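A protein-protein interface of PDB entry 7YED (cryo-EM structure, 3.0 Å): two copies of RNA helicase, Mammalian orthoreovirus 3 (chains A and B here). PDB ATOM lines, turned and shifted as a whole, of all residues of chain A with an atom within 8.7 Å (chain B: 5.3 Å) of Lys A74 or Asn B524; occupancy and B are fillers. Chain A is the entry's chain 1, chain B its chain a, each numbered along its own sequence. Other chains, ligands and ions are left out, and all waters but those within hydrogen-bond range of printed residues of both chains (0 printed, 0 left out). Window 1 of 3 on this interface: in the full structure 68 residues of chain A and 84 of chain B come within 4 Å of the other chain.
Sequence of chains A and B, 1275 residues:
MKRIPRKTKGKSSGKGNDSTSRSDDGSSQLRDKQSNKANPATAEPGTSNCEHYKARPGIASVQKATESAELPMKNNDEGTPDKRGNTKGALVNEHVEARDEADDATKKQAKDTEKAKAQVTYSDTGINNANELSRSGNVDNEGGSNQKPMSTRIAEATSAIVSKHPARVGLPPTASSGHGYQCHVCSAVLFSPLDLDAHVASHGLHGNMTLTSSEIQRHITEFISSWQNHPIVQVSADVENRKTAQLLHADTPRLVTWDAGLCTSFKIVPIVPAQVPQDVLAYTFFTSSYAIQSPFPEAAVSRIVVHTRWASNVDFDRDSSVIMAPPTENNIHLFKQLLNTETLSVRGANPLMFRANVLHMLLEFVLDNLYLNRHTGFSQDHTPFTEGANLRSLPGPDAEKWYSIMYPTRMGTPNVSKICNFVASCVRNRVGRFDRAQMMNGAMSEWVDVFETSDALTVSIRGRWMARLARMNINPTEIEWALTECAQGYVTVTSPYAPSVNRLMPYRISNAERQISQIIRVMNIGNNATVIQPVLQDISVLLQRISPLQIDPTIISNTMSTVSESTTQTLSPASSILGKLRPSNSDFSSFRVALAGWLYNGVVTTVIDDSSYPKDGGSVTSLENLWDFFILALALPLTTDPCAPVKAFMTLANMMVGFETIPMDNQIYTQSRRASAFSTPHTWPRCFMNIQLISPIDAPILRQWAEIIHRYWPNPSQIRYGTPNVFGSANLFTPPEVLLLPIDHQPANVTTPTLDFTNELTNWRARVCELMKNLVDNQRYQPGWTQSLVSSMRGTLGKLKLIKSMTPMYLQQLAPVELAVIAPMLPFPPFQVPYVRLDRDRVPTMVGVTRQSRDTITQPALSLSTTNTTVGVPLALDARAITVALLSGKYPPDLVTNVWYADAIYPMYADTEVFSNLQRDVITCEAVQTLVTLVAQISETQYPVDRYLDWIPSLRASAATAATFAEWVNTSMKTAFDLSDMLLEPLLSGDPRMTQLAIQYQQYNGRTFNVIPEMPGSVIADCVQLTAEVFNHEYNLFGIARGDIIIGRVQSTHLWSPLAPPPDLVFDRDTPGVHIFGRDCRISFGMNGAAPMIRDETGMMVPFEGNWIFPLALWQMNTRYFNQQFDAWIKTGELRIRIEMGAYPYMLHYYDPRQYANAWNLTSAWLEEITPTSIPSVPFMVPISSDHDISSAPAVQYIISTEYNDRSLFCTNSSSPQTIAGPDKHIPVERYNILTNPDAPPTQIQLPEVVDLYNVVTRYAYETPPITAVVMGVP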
ATOM      1  N   LEU A  71     -12.169 -30.795  16.113  1.00  0.00           N
ATOM      2  CA  LEU A  71     -10.807 -30.657  16.613  1.00  0.00           C
ATOM      3  C   LEU A  71     -10.711 -29.522  17.628  1.00  0.00           C
ATOM      4  O   LEU A  71     -11.361 -28.486  17.469  1.00  0.00           O
ATOM      5  CB  LEU A  71      -9.829 -30.392  15.472  1.00  0.00           C
ATOM      6  CG  LEU A  71      -9.350 -31.568  14.629  1.00  0.00           C
ATOM      7  CD1 LEU A  71     -10.453 -32.048  13.726  1.00  0.00           C
ATOM      8  CD2 LEU A  71      -8.143 -31.152  13.812  1.00  0.00           C
ATOM      9  N   PRO A  72      -9.905 -29.683  18.673  1.00  0.00           N
ATOM     10  CA  PRO A  72      -9.699 -28.583  19.618  1.00  0.00           C
ATOM     11  C   PRO A  72      -8.961 -27.427  18.968  1.00  0.00           C
ATOM     12  O   PRO A  72      -8.176 -27.602  18.035  1.00  0.00           O
ATOM     13  CB  PRO A  72      -8.857 -29.221  20.728  1.00  0.00           C
ATOM     14  CG  PRO A  72      -9.118 -30.677  20.612  1.00  0.00           C
ATOM     15  CD  PRO A  72      -9.285 -30.928  19.144  1.00  0.00           C
ATOM     16  N   MET A  73      -9.225 -26.233  19.486  1.00  0.00           N
ATOM     17  CA  MET A  73      -8.624 -25.022  18.949  1.00  0.00           C
ATOM     18  C   MET A  73      -7.106 -25.058  19.107  1.00  0.00           C
ATOM     19  O   MET A  73      -6.567 -25.743  19.977  1.00  0.00           O
ATOM     20  CB  MET A  73      -9.214 -23.803  19.658  1.00  0.00           C
ATOM     21  CG  MET A  73      -8.734 -22.463  19.149  1.00  0.00           C
ATOM     22  SD  MET A  73      -9.543 -21.108  20.015  1.00  0.00           S
ATOM     23  CE  MET A  73      -8.785 -21.249  21.628  1.00  0.00           C
ATOM     24  N   LYS A  74      -6.418 -24.316  18.241  1.00  0.00           N
ATOM     25  CA  LYS A  74      -4.962 -24.268  18.260  1.00  0.00           C
ATOM     26  C   LYS A  74      -4.466 -23.693  19.586  1.00  0.00           C
ATOM     27  O   LYS A  74      -5.196 -23.020  20.315  1.00  0.00           O
ATOM     28  CB  LYS A  74      -4.454 -23.432  17.085  1.00  0.00           C
ATOM     29  CG  LYS A  74      -2.946 -23.363  16.930  1.00  0.00           C
ATOM     30  CD  LYS A  74      -2.565 -22.592  15.680  1.00  0.00           C
ATOM     31  CE  LYS A  74      -1.067 -22.363  15.599  1.00  0.00           C
ATOM     32  NZ  LYS A  74      -0.315 -23.634  15.419  1.00  0.00           N
ATOM     33  N   ASN A  75      -3.206 -23.977  19.899  1.00  0.00           N
ATOM     34  CA  ASN A  75      -2.566 -23.528  21.135  1.00  0.00           C
ATOM     35  C   ASN A  75      -1.576 -22.418  20.795  1.00  0.00           C
ATOM     36  O   ASN A  75      -0.396 -22.673  20.560  1.00  0.00           O
ATOM     37  CB  ASN A  75      -1.869 -24.683  21.838  1.00  0.00           C
ATOM     38  CG  ASN A  75      -1.352 -24.301  23.208  1.00  0.00           C
ATOM     39  OD1 ASN A  75      -1.509 -23.165  23.650  1.00  0.00           O
ATOM     40  ND2 ASN A  75      -0.726 -25.251  23.889  1.00  0.00           N
ATOM     41  N   ASN A  76      -2.062 -21.182  20.778  1.00  0.00           N
ATOM     42  CA  ASN A  76      -1.180 -20.041  20.588  1.00  0.00           C
ATOM     43  C   ASN A  76      -0.234 -19.937  21.776  1.00  0.00           C
ATOM     44  O   ASN A  76      -0.670 -19.943  22.930  1.00  0.00           O
ATOM     45  CB  ASN A  76      -1.994 -18.762  20.428  1.00  0.00           C
ATOM     46  CG  ASN A  76      -1.157 -17.596  19.964  1.00  0.00           C
ATOM     47  OD1 ASN A  76       0.054 -17.715  19.796  1.00  0.00           O
ATOM     48  ND2 ASN A  76      -1.800 -16.457  19.748  1.00  0.00           N
ATOM     49  N   ASP A  77       1.064 -19.853  21.496  1.00  0.00           N
ATOM     50  CA  ASP A  77       2.057 -20.038  22.544  1.00  0.00           C
ATOM     51  C   ASP A  77       3.104 -18.932  22.539  1.00  0.00           C
ATOM     52  O   ASP A  77       3.701 -18.635  23.578  1.00  0.00           O
ATOM     53  CB  ASP A  77       2.730 -21.399  22.376  1.00  0.00           C
ATOM     54  CG  ASP A  77       3.537 -21.804  23.585  1.00  0.00           C
ATOM     55  OD1 ASP A  77       3.562 -21.043  24.570  1.00  0.00           O
ATOM     56  OD2 ASP A  77       4.150 -22.891  23.547  1.00  0.00           O
ATOM     57  N   GLU A  78       3.324 -18.319  21.379  1.00  0.00           N
ATOM     58  CA  GLU A  78       4.404 -17.352  21.222  1.00  0.00           C
ATOM     59  C   GLU A  78       4.212 -16.170  22.159  1.00  0.00           C
ATOM     60  O   GLU A  78       3.199 -15.469  22.090  1.00  0.00           O
ATOM     61  CB  GLU A  78       4.475 -16.875  19.774  1.00  0.00           C
ATOM     62  CG  GLU A  78       4.913 -17.946  18.787  1.00  0.00           C
ATOM     63  CD  GLU A  78       4.981 -17.437  17.359  1.00  0.00           C
ATOM     64  OE1 GLU A  78       4.577 -16.282  17.117  1.00  0.00           O
ATOM     65  OE2 GLU A  78       5.437 -18.195  16.477  1.00  0.00           O
ATOM     66  N   THR A  80       5.230 -16.601  25.739  1.00  0.00           N
ATOM     67  CA  THR A  80       5.171 -17.077  27.108  1.00  0.00           C
ATOM     68  C   THR A  80       6.460 -17.800  27.477  1.00  0.00           C
ATOM     69  O   THR A  80       7.101 -18.411  26.618  1.00  0.00           O
ATOM     70  CB  THR A  80       3.985 -18.024  27.308  1.00  0.00           C
ATOM     71  OG1 THR A  80       4.152 -19.179  26.481  1.00  0.00           O
ATOM     72  CG2 THR A  80       2.696 -17.327  26.925  1.00  0.00           C
ATOM     73  N   LYS A 108      -3.688 -20.901   3.928  1.00  0.00           N
ATOM     74  CA  LYS A 108      -4.305 -22.137   4.398  1.00  0.00           C
ATOM     75  C   LYS A 108      -5.764 -22.227   3.967  1.00  0.00           C
ATOM     76  O   LYS A 108      -6.252 -23.311   3.630  1.00  0.00           O
ATOM     77  CB  LYS A 108      -4.186 -22.240   5.914  1.00  0.00           C
ATOM     78  CG  LYS A 108      -4.750 -23.524   6.477  1.00  0.00           C
ATOM     79  CD  LYS A 108      -3.932 -24.721   6.033  1.00  0.00           C
ATOM     80  CE  LYS A 108      -4.510 -26.010   6.581  1.00  0.00           C
ATOM     81  NZ  LYS A 108      -4.399 -26.077   8.062  1.00  0.00           N
ATOM     82  N   ARG A 135       1.354 -11.640  19.690  1.00  0.00           N
ATOM     83  CA  ARG A 135       2.338 -12.008  20.696  1.00  0.00           C
ATOM     84  C   ARG A 135       3.494 -12.727  20.016  1.00  0.00           C
ATOM     85  O   ARG A 135       3.297 -13.763  19.375  1.00  0.00           O
ATOM     86  CB  ARG A 135       1.701 -12.878  21.775  1.00  0.00           C
ATOM     87  CG  ARG A 135       0.712 -12.126  22.642  1.00  0.00           C
ATOM     88  CD  ARG A 135       0.152 -12.991  23.751  1.00  0.00           C
ATOM     89  NE  ARG A 135      -0.734 -14.029  23.238  1.00  0.00           N
ATOM     90  CZ  ARG A 135      -0.464 -15.328  23.294  1.00  0.00           C
ATOM     91  NH1 ARG A 135       0.667 -15.747  23.840  1.00  0.00           N
ATOM     92  NH2 ARG A 135      -1.323 -16.206  22.805  1.00  0.00           N
ATOM     93  N   ILE B 519     -13.488 -17.127  28.709  1.00  0.00           N
ATOM     94  CA  ILE B 519     -12.611 -15.961  28.703  1.00  0.00           C
ATOM     95  C   ILE B 519     -11.187 -16.370  28.360  1.00  0.00           C
ATOM     96  O   ILE B 519     -10.491 -15.673  27.612  1.00  0.00           O
ATOM     97  CB  ILE B 519     -12.668 -15.225  30.050  1.00  0.00           C
ATOM     98  CG1 ILE B 519     -14.061 -14.665  30.298  1.00  0.00           C
ATOM     99  CG2 ILE B 519     -11.660 -14.105  30.068  1.00  0.00           C
ATOM    100  CD1 ILE B 519     -14.246 -14.137  31.692  1.00  0.00           C
ATOM    101  N   ILE B 520     -10.727 -17.499  28.906  1.00  0.00           N
ATOM    102  CA  ILE B 520      -9.395 -17.988  28.552  1.00  0.00           C
ATOM    103  C   ILE B 520      -9.313 -18.275  27.059  1.00  0.00           C
ATOM    104  O   ILE B 520      -8.326 -17.928  26.395  1.00  0.00           O
ATOM    105  CB  ILE B 520      -9.031 -19.230  29.381  1.00  0.00           C
ATOM    106  CG1 ILE B 520      -9.032 -18.904  30.870  1.00  0.00           C
ATOM    107  CG2 ILE B 520      -7.670 -19.737  28.979  1.00  0.00           C
ATOM    108  CD1 ILE B 520      -8.010 -17.881  31.257  1.00  0.00           C
ATOM    109  N   ARG B 521     -10.350 -18.904  26.503  1.00  0.00           N
ATOM    110  CA  ARG B 521     -10.351 -19.182  25.071  1.00  0.00           C
ATOM    111  C   ARG B 521     -10.298 -17.898  24.253  1.00  0.00           C
ATOM    112  O   ARG B 521      -9.543 -17.805  23.282  1.00  0.00           O
ATOM    113  CB  ARG B 521     -11.585 -19.988  24.683  1.00  0.00           C
ATOM    114  CG  ARG B 521     -11.629 -21.408  25.174  1.00  0.00           C
ATOM    115  CD  ARG B 521     -12.894 -22.069  24.676  1.00  0.00           C
ATOM    116  NE  ARG B 521     -13.017 -23.444  25.136  1.00  0.00           N
ATOM    117  CZ  ARG B 521     -13.617 -23.790  26.267  1.00  0.00           C
ATOM    118  NH1 ARG B 521     -14.140 -22.860  27.052  1.00  0.00           N
ATOM    119  NH2 ARG B 521     -13.690 -25.065  26.617  1.00  0.00           N
ATOM    120  N   VAL B 522     -11.102 -16.901  24.628  1.00  0.00           N
ATOM    121  CA  VAL B 522     -11.128 -15.644  23.882  1.00  0.00           C
ATOM    122  C   VAL B 522      -9.777 -14.953  23.956  1.00  0.00           C
ATOM    123  O   VAL B 522      -9.316 -14.350  22.979  1.00  0.00           O
ATOM    124  CB  VAL B 522     -12.248 -14.731  24.406  1.00  0.00           C
ATOM    125  CG1 VAL B 522     -12.184 -13.389  23.714  1.00  0.00           C
ATOM    126  CG2 VAL B 522     -13.594 -15.375  24.190  1.00  0.00           C
ATOM    127  N   MET B 523      -9.125 -15.020  25.113  1.00  0.00           N
ATOM    128  CA  MET B 523      -7.823 -14.390  25.266  1.00  0.00           C
ATOM    129  C   MET B 523      -6.724 -15.166  24.554  1.00  0.00           C
ATOM    130  O   MET B 523      -5.657 -14.605  24.292  1.00  0.00           O
ATOM    131  CB  MET B 523      -7.511 -14.247  26.751  1.00  0.00           C
ATOM    132  CG  MET B 523      -6.225 -13.538  27.067  1.00  0.00           C
ATOM    133  SD  MET B 523      -6.025 -13.403  28.849  1.00  0.00           S
ATOM    134  CE  MET B 523      -5.739 -15.117  29.261  1.00  0.00           C
ATOM    135  N   ASN B 524      -6.961 -16.442  24.245  1.00  0.00           N
ATOM    136  CA  ASN B 524      -5.979 -17.218  23.492  1.00  0.00           C
ATOM    137  C   ASN B 524      -5.709 -16.620  22.119  1.00  0.00           C
ATOM    138  O   ASN B 524      -4.559 -16.603  21.665  1.00  0.00           O
ATOM    139  CB  ASN B 524      -6.458 -18.658  23.332  1.00  0.00           C
ATOM    140  CG  ASN B 524      -5.415 -19.553  22.700  1.00  0.00           C
ATOM    141  OD1 ASN B 524      -4.290 -19.134  22.439  1.00  0.00           O
ATOM    142  ND2 ASN B 524      -5.788 -20.794  22.443  1.00  0.00           N
ATOM    143  N   ILE B 525      -6.755 -16.150  21.435  1.00  0.00           N
ATOM    144  CA  ILE B 525      -6.652 -15.810  20.014  1.00  0.00           C
ATOM    145  C   ILE B 525      -5.603 -14.729  19.792  1.00  0.00           C
ATOM    146  O   ILE B 525      -4.606 -14.942  19.096  1.00  0.00           O
ATOM    147  CB  ILE B 525      -8.022 -15.384  19.463  1.00  0.00           C
ATOM    148  CG1 ILE B 525      -8.998 -16.553  19.523  1.00  0.00           C
ATOM    149  CG2 ILE B 525      -7.893 -14.893  18.045  1.00  0.00           C
ATOM    150  CD1 ILE B 525     -10.411 -16.161  19.222  1.00  0.00           C
ATOM    151  N   GLY B 526      -5.808 -13.559  20.386  1.00  0.00           N
ATOM    152  CA  GLY B 526      -4.805 -12.513  20.350  1.00  0.00           C
ATOM    153  C   GLY B 526      -4.450 -12.023  18.963  1.00  0.00           C
ATOM    154  O   GLY B 526      -3.270 -11.908  18.623  1.00  0.00           O
ATOM    155  N   THR B 530      -4.718 -17.211  12.258  1.00  0.00           N
ATOM    156  CA  THR B 530      -4.453 -18.630  12.078  1.00  0.00           C
ATOM    157  C   THR B 530      -5.181 -19.481  13.107  1.00  0.00           C
ATOM    158  O   THR B 530      -5.410 -20.670  12.864  1.00  0.00           O
ATOM    159  CB  THR B 530      -2.949 -18.894  12.150  1.00  0.00           C
ATOM    160  OG1 THR B 530      -2.285 -18.130  11.140  1.00  0.00           O
ATOM    161  CG2 THR B 530      -2.653 -20.360  11.925  1.00  0.00           C
ATOM    162  N   VAL B 531      -5.558 -18.900  14.244  1.00  0.00           N
ATOM    163  CA  VAL B 531      -6.283 -19.644  15.263  1.00  0.00           C
ATOM    164  C   VAL B 531      -7.782 -19.696  14.992  1.00  0.00           C
ATOM    165  O   VAL B 531      -8.453 -20.628  15.456  1.00  0.00           O
ATOM    166  CB  VAL B 531      -6.019 -19.042  16.652  1.00  0.00           C
ATOM    167  CG1 VAL B 531      -6.815 -19.767  17.711  1.00  0.00           C
ATOM    168  CG2 VAL B 531      -4.545 -19.097  16.975  1.00  0.00           C
ATOM    169  N   MET B 982      -3.316 -26.575  25.523  1.00  0.00           N
ATOM    170  CA  MET B 982      -3.265 -25.324  26.261  1.00  0.00           C
ATOM    171  C   MET B 982      -4.033 -25.428  27.569  1.00  0.00           C
ATOM    172  O   MET B 982      -5.103 -26.037  27.638  1.00  0.00           O
ATOM    173  CB  MET B 982      -3.846 -24.191  25.426  1.00  0.00           C
ATOM    174  CG  MET B 982      -3.806 -22.866  26.137  1.00  0.00           C
ATOM    175  SD  MET B 982      -4.596 -21.572  25.187  1.00  0.00           S
ATOM    176  CE  MET B 982      -6.307 -22.055  25.362  1.00  0.00           C
ATOM    177  N   PRO B 986      -2.439 -18.622  28.104  1.00  0.00           N
ATOM    178  CA  PRO B 986      -2.664 -17.217  27.729  1.00  0.00           C
ATOM    179  C   PRO B 986      -2.477 -16.241  28.875  1.00  0.00           C
ATOM    180  O   PRO B 986      -2.176 -15.067  28.631  1.00  0.00           O
ATOM    181  CB  PRO B 986      -4.110 -17.220  27.225  1.00  0.00           C
ATOM    182  CG  PRO B 986      -4.325 -18.584  26.747  1.00  0.00           C
ATOM    183  CD  PRO B 986      -3.562 -19.471  27.669  1.00  0.00           C
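Of chain B, only Asn B524 comes within 4 Å of Lys A74. Of chain A, only Met A73 (3.1 Å), Lys A74 (3.1 Å), Asn A76 (3.1 Å) and Arg A135 (3.5 Å) come within 4 Å of Asn B524. Of the printed residues of chain A, Met B982 touches Asn A75 (3.1 Å). Of the printed residues of chain A, Ile B525 touches Asn A76 (3.3 Å). Printed residues of chain B within 4 Å of Asn A75: Met B982. Of the printed residues of chain B, Met A73 touches Arg B521 (3.9 Å), Asn B524 (3.1 Å) and Val B531 (3.6 Å). Ile B519 touches none of the printed residues of chain A. Thr B530 touches none of the printed residues of chain A. The nearest residue of chain A that does not touch Asn B524 is Asn A75 (4.4 Å).
Among the printed residues, merely in contact across the chains: Met A73 with Asn B524 (3.1 Å), Met A73 with Val B531 (3.6 Å) and Met A73 with Arg B521 (3.9 Å).
O of Glu A78 lies close to NH1 of Arg A135 (3.1 Å). ND2 of Asn A76 sits close to NH2 of Arg A135 (3.1 Å). The side-chain sulfur of Met B982 sits at hydrogen-bond distance from the side-chain amide nitrogen of Asn B524 (3.1 Å).
The backbone carbonyl oxygen (O) of Asn B524 is in hydrogen-bond range of the side-chain amide nitrogen (ND2) of Asn A76 (3.4 Å). O of Asn B524 is in hydrogen-bond range of NH2 of Arg A135. The side-chain amide nitrogen (ND2) of Asn A76 sits at hydrogen-bond distance from the backbone carbonyl oxygen (O) of Ile B525 (3.3 Å). The side-chain amide nitrogen of Asn B524 is in hydrogen-bond range of the backbone carbonyl oxygen of Lys A74 (3.1 Å). N of Met B982 sits close to ND2 of Asn A75, 3.3 Å away.
No position is printed for both chains.
Of the 11 printed residues of chain A, 5 touch a printed residue of chain B. Of the 12 printed residues of chain B, 5 touch a printed residue of chain A.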
